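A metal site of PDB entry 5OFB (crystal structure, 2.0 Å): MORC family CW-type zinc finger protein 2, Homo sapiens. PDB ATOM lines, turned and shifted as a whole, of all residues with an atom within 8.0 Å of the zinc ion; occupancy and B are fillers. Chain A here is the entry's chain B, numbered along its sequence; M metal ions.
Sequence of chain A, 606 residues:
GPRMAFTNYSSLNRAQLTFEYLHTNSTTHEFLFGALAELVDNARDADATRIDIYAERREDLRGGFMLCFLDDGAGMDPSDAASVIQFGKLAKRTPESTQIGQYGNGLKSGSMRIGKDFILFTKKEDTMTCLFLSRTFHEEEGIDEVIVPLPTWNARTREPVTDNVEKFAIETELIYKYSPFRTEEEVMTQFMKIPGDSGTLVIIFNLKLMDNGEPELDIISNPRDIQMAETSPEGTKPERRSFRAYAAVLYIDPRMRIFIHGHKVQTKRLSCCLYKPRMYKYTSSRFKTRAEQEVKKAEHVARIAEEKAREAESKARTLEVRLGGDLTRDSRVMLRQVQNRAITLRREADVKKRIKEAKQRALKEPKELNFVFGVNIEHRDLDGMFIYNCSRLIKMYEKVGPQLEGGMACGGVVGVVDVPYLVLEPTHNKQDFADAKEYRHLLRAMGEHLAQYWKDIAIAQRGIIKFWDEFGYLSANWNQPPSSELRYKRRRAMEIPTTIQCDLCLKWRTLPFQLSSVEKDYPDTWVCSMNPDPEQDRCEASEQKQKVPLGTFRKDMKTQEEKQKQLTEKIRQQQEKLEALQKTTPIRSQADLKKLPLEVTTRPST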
ATOM      1  N   GLN A 501       2.442   4.599  24.176  1.00  0.00           N
ATOM      2  CA  GLN A 501       2.845   5.355  23.020  1.00  0.00           C
ATOM      3  C   GLN A 501       2.486   6.800  23.161  1.00  0.00           C
ATOM      4  O   GLN A 501       1.372   7.118  23.516  1.00  0.00           O
ATOM      5  CB  GLN A 501       2.188   4.819  21.732  1.00  0.00           C
ATOM      6  CG  GLN A 501       2.713   5.478  20.467  1.00  0.00           C
ATOM      7  CD  GLN A 501       2.083   4.954  19.185  1.00  0.00           C
ATOM      8  OE1 GLN A 501       0.963   4.411  19.212  1.00  0.00           O
ATOM      9  NE2 GLN A 501       2.785   5.097  18.080  1.00  0.00           N
ATOM     10  N   CYS A 502       3.420   7.680  22.833  1.00  0.00           N
ATOM     11  CA  CYS A 502       3.156   9.105  22.856  1.00  0.00           C
ATOM     12  C   CYS A 502       2.246   9.546  21.727  1.00  0.00           C
ATOM     13  O   CYS A 502       2.493   9.289  20.548  1.00  0.00           O
ATOM     14  CB  CYS A 502       4.467   9.913  22.812  1.00  0.00           C
ATOM     15  SG  CYS A 502       4.266  11.713  22.746  1.00  0.00           S
ATOM     16  N   ASP A 503       1.203  10.260  22.062  1.00  0.00           N
ATOM     17  CA  ASP A 503       0.254  10.763  21.055  1.00  0.00           C
ATOM     18  C   ASP A 503       0.784  11.831  20.129  1.00  0.00           C
ATOM     19  O   ASP A 503       0.201  12.081  19.075  1.00  0.00           O
ATOM     20  CB  ASP A 503      -1.008  11.333  21.676  1.00  0.00           C
ATOM     21  CG  ASP A 503      -2.103  10.355  21.682  1.00  0.00           C
ATOM     22  OD1 ASP A 503      -2.746   9.962  20.670  1.00  0.00           O
ATOM     23  OD2 ASP A 503      -2.299  10.023  22.874  1.00  0.00           O
ATOM     24  N   LEU A 504       1.864  12.490  20.521  1.00  0.00           N
ATOM     25  CA  LEU A 504       2.461  13.576  19.710  1.00  0.00           C
ATOM     26  C   LEU A 504       3.546  13.114  18.731  1.00  0.00           C
ATOM     27  O   LEU A 504       3.500  13.441  17.535  1.00  0.00           O
ATOM     28  CB  LEU A 504       3.090  14.648  20.628  1.00  0.00           C
ATOM     29  CG  LEU A 504       2.114  15.468  21.445  1.00  0.00           C
ATOM     30  CD1 LEU A 504       2.909  16.398  22.349  1.00  0.00           C
ATOM     31  CD2 LEU A 504       1.218  16.277  20.526  1.00  0.00           C
ATOM     32  N   CYS A 505       4.534  12.388  19.236  1.00  0.00           N
ATOM     33  CA  CYS A 505       5.699  11.996  18.462  1.00  0.00           C
ATOM     34  C   CYS A 505       5.692  10.509  18.058  1.00  0.00           C
ATOM     35  O   CYS A 505       6.580  10.081  17.298  1.00  0.00           O
ATOM     36  CB  CYS A 505       6.984  12.352  19.251  1.00  0.00           C
ATOM     37  SG  CYS A 505       7.366  11.239  20.629  1.00  0.00           S
ATOM     38  N   LEU A 506       4.758   9.729  18.592  1.00  0.00           N
ATOM     39  CA  LEU A 506       4.536   8.333  18.223  1.00  0.00           C
ATOM     40  C   LEU A 506       5.574   7.355  18.770  1.00  0.00           C
ATOM     41  O   LEU A 506       5.532   6.168  18.450  1.00  0.00           O
ATOM     42  CB  LEU A 506       4.452   8.140  16.706  1.00  0.00           C
ATOM     43  CG  LEU A 506       3.240   8.744  16.026  1.00  0.00           C
ATOM     44  CD1 LEU A 506       3.534   8.832  14.576  1.00  0.00           C
ATOM     45  CD2 LEU A 506       1.845   8.321  16.390  1.00  0.00           C
ATOM     46  N   LYS A 507       6.526   7.835  19.576  1.00  0.00           N
ATOM     47  CA  LYS A 507       7.494   6.935  20.180  1.00  0.00           C
ATOM     48  C   LYS A 507       6.869   6.067  21.251  1.00  0.00           C
ATOM     49  O   LYS A 507       5.896   6.469  21.943  1.00  0.00           O
ATOM     50  CB  LYS A 507       8.665   7.717  20.772  1.00  0.00           C
ATOM     51  CG  LYS A 507       9.535   8.418  19.744  1.00  0.00           C
ATOM     52  CD  LYS A 507      10.656   9.241  20.412  1.00  0.00           C
ATOM     53  CE  LYS A 507      11.389  10.115  19.395  1.00  0.00           C
ATOM     54  NZ  LYS A 507      10.766  11.400  19.184  1.00  0.00           N
ATOM     55  N   TRP A 508       7.431   4.884  21.433  1.00  0.00           N
ATOM     56  CA  TRP A 508       7.041   3.958  22.469  1.00  0.00           C
ATOM     57  C   TRP A 508       7.939   4.139  23.707  1.00  0.00           C
ATOM     58  O   TRP A 508       9.174   4.218  23.595  1.00  0.00           O
ATOM     59  CB  TRP A 508       7.141   2.511  21.937  1.00  0.00           C
ATOM     60  CG  TRP A 508       5.914   2.150  21.100  1.00  0.00           C
ATOM     61  CD1 TRP A 508       5.803   2.192  19.740  1.00  0.00           C
ATOM     62  CD2 TRP A 508       4.642   1.725  21.598  1.00  0.00           C
ATOM     63  NE1 TRP A 508       4.565   1.807  19.383  1.00  0.00           N
ATOM     64  CE2 TRP A 508       3.820   1.499  20.487  1.00  0.00           C
ATOM     65  CE3 TRP A 508       4.122   1.530  22.856  1.00  0.00           C
ATOM     66  CZ2 TRP A 508       2.497   1.105  20.602  1.00  0.00           C
ATOM     67  CZ3 TRP A 508       2.805   1.079  22.969  1.00  0.00           C
ATOM     68  CH2 TRP A 508       2.017   0.877  21.844  1.00  0.00           C
ATOM     69  N   ARG A 509       7.306   4.265  24.875  1.00  0.00           N
ATOM     70  CA  ARG A 509       7.967   4.519  26.131  1.00  0.00           C
ATOM     71  C   ARG A 509       7.640   3.415  27.134  1.00  0.00           C
ATOM     72  O   ARG A 509       6.628   2.752  26.997  1.00  0.00           O
ATOM     73  CB  ARG A 509       7.489   5.857  26.722  1.00  0.00           C
ATOM     74  CG  ARG A 509       7.734   7.070  25.840  1.00  0.00           C
ATOM     75  CD  ARG A 509       9.221   7.227  25.493  1.00  0.00           C
ATOM     76  NE  ARG A 509       9.501   8.518  24.870  1.00  0.00           N
ATOM     77  CZ  ARG A 509      10.654   8.837  24.296  1.00  0.00           C
ATOM     78  NH1 ARG A 509      11.641   7.965  24.224  1.00  0.00           N
ATOM     79  NH2 ARG A 509      10.817  10.034  23.781  1.00  0.00           N
ATOM     80  N   TRP A 526      -1.803  10.428  26.141  1.00  0.00           N
ATOM     81  CA  TRP A 526      -0.547  10.357  26.872  1.00  0.00           C
ATOM     82  C   TRP A 526       0.544  10.927  25.977  1.00  0.00           C
ATOM     83  O   TRP A 526       0.609  10.637  24.766  1.00  0.00           O
ATOM     84  CB  TRP A 526      -0.221   8.922  27.276  1.00  0.00           C
ATOM     85  CG  TRP A 526       0.915   8.828  28.240  1.00  0.00           C
ATOM     86  CD1 TRP A 526       0.844   8.846  29.598  1.00  0.00           C
ATOM     87  CD2 TRP A 526       2.291   8.709  27.901  1.00  0.00           C
ATOM     88  NE1 TRP A 526       2.106   8.742  30.126  1.00  0.00           N
ATOM     89  CE2 TRP A 526       3.012   8.638  29.095  1.00  0.00           C
ATOM     90  CE3 TRP A 526       2.985   8.631  26.683  1.00  0.00           C
ATOM     91  CZ2 TRP A 526       4.406   8.524  29.138  1.00  0.00           C
ATOM     92  CZ3 TRP A 526       4.343   8.489  26.707  1.00  0.00           C
ATOM     93  CH2 TRP A 526       5.063   8.455  27.933  1.00  0.00           C
ATOM     94  N   VAL A 527       1.405  11.726  26.575  1.00  0.00           N
ATOM     95  CA  VAL A 527       2.565  12.258  25.868  1.00  0.00           C
ATOM     96  C   VAL A 527       3.824  12.059  26.702  1.00  0.00           C
ATOM     97  O   VAL A 527       3.761  11.828  27.918  1.00  0.00           O
ATOM     98  CB  VAL A 527       2.397  13.747  25.532  1.00  0.00           C
ATOM     99  CG1 VAL A 527       1.196  13.903  24.618  1.00  0.00           C
ATOM    100  CG2 VAL A 527       2.256  14.573  26.824  1.00  0.00           C
ATOM    101  N   CYS A 528       4.968  12.168  26.036  1.00  0.00           N
ATOM    102  CA  CYS A 528       6.239  11.824  26.667  1.00  0.00           C
ATOM    103  C   CYS A 528       6.463  12.616  27.995  1.00  0.00           C
ATOM    104  O   CYS A 528       6.999  12.067  28.977  1.00  0.00           O
ATOM    105  CB  CYS A 528       7.393  12.097  25.697  1.00  0.00           C
ATOM    106  SG  CYS A 528       7.435  10.980  24.271  1.00  0.00           S
ATOM    107  N   SER A 529       6.083  13.895  28.043  1.00  0.00           N
ATOM    108  CA  SER A 529       6.409  14.705  29.219  1.00  0.00           C
ATOM    109  C   SER A 529       5.647  14.284  30.477  1.00  0.00           C
ATOM    110  O   SER A 529       5.985  14.684  31.545  1.00  0.00           O
ATOM    111  CB  SER A 529       6.180  16.191  28.960  1.00  0.00           C
ATOM    112  OG  SER A 529       4.798  16.415  28.685  1.00  0.00           O
ATOM    113  N   GLN A 536      13.256   9.470  29.560  1.00  0.00           N
ATOM    114  CA  GLN A 536      12.294   9.325  28.455  1.00  0.00           C
ATOM    115  C   GLN A 536      11.213  10.400  28.516  1.00  0.00           C
ATOM    116  O   GLN A 536      10.122  10.230  27.958  1.00  0.00           O
ATOM    117  CB  GLN A 536      11.575   7.979  28.522  1.00  0.00           C
ATOM    118  CG  GLN A 536      12.398   6.813  28.967  1.00  0.00           C
ATOM    119  CD  GLN A 536      11.546   5.546  29.037  1.00  0.00           C
ATOM    120  OE1 GLN A 536      11.008   5.090  28.028  1.00  0.00           O
ATOM    121  NE2 GLN A 536      11.414   4.995  30.226  1.00  0.00           N
ATOM    122  N   ASP A 537      11.532  11.500  29.186  1.00  0.00           N
ATOM    123  CA  ASP A 537      10.518  12.429  29.601  1.00  0.00           C
ATOM    124  C   ASP A 537      10.263  13.609  28.658  1.00  0.00           C
ATOM    125  O   ASP A 537       9.633  14.600  29.035  1.00  0.00           O
ATOM    126  CB  ASP A 537      10.480  12.708  31.114  1.00  0.00           C
ATOM    127  CG  ASP A 537      11.194  13.896  31.572  1.00  0.00           C
ATOM    128  OD1 ASP A 537      12.171  14.156  30.821  1.00  0.00           O
ATOM    129  OD2 ASP A 537      11.064  14.423  32.707  1.00  0.00           O
ATOM    130  N   ARG A 538      10.723  13.479  27.431  1.00  0.00           N
ATOM    131  CA  ARG A 538      10.584  14.528  26.444  1.00  0.00           C
ATOM    132  C   ARG A 538      10.454  13.823  25.105  1.00  0.00           C
ATOM    133  O   ARG A 538      11.075  12.795  24.881  1.00  0.00           O
ATOM    134  CB  ARG A 538      11.865  15.385  26.404  1.00  0.00           C
ATOM    135  CG  ARG A 538      12.196  16.185  27.630  1.00  0.00           C
ATOM    136  CD  ARG A 538      13.646  16.677  27.555  1.00  0.00           C
ATOM    137  NE  ARG A 538      13.919  17.539  26.389  1.00  0.00           N
ATOM    138  CZ  ARG A 538      14.928  18.417  26.300  1.00  0.00           C
ATOM    139  NH1 ARG A 538      15.792  18.603  27.313  1.00  0.00           N
ATOM    140  NH2 ARG A 538      15.065  19.146  25.184  1.00  0.00           N
ATOM    141  N   CYS A 539       9.716  14.395  24.183  1.00  0.00           N
ATOM    142  CA  CYS A 539       9.572  13.814  22.867  1.00  0.00           C
ATOM    143  C   CYS A 539      10.928  13.713  22.148  1.00  0.00           C
ATOM    144  O   CYS A 539      11.134  12.840  21.322  1.00  0.00           O
ATOM    145  CB  CYS A 539       8.585  14.605  22.010  1.00  0.00           C
ATOM    146  SG  CYS A 539       6.892  14.456  22.570  1.00  0.00           S
ATOM    147  N   GLU A 540      11.876  14.570  22.489  1.00  0.00           N
ATOM    148  CA  GLU A 540      13.145  14.569  21.826  1.00  0.00           C
ATOM    149  C   GLU A 540      14.048  13.435  22.350  1.00  0.00           C
ATOM    150  O   GLU A 540      15.040  13.139  21.698  1.00  0.00           O
ATOM    151  CB  GLU A 540      13.902  15.882  22.041  1.00  0.00           C
ATOM    152  CG  GLU A 540      13.241  17.163  21.540  1.00  0.00           C
ATOM    153  CD  GLU A 540      11.977  17.551  22.314  1.00  0.00           C
ATOM    154  OE1 GLU A 540      11.811  17.369  23.544  1.00  0.00           O
ATOM    155  OE2 GLU A 540      11.057  17.996  21.676  1.00  0.00           O
ATOM    156  N   ALA A 541      13.760  12.863  23.514  1.00  0.00           N
ATOM    157  CA  ALA A 541      14.561  11.713  24.010  1.00  0.00           C
ATOM    158  C   ALA A 541      14.411  10.557  23.024  1.00  0.00           C
ATOM    159  O   ALA A 541      13.296  10.215  22.614  1.00  0.00           O
ATOM    160  CB  ALA A 541      14.095  11.275  25.375  1.00  0.00           C
HETATM  161 ZN    ZN M   1       6.541  12.174  22.561  1.00  0.00          ZN
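NE of Arg 509 lies close to SG of Cys 528, 3.3 Å away. The backbone NH (N) of Lys 507 sits close to the side-chain sulfur (SG) of Cys 505, 3.7 Å away. The backbone carbonyl oxygen (O) of Cys 539 is in hydrogen-bond range of the side-chain amino group (NZ) of Lys 507 (2.6 Å). N of Leu 504 lies close to SG of Cys 502. The backbone carbonyl oxygen (O) of Lys 507 is in hydrogen-bond range of the backbone NH (N) of Cys 502 (2.9 Å).
The zinc ion is bound by SG of Cys 528 (2.3 Å), SG of Cys 505 (2.3 Å), SG of Cys 539 (2.3 Å) and SG of Cys 502 (2.3 Å).
Along chain A the residues within 4 Å of the zinc ion span positions 502 to 539.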
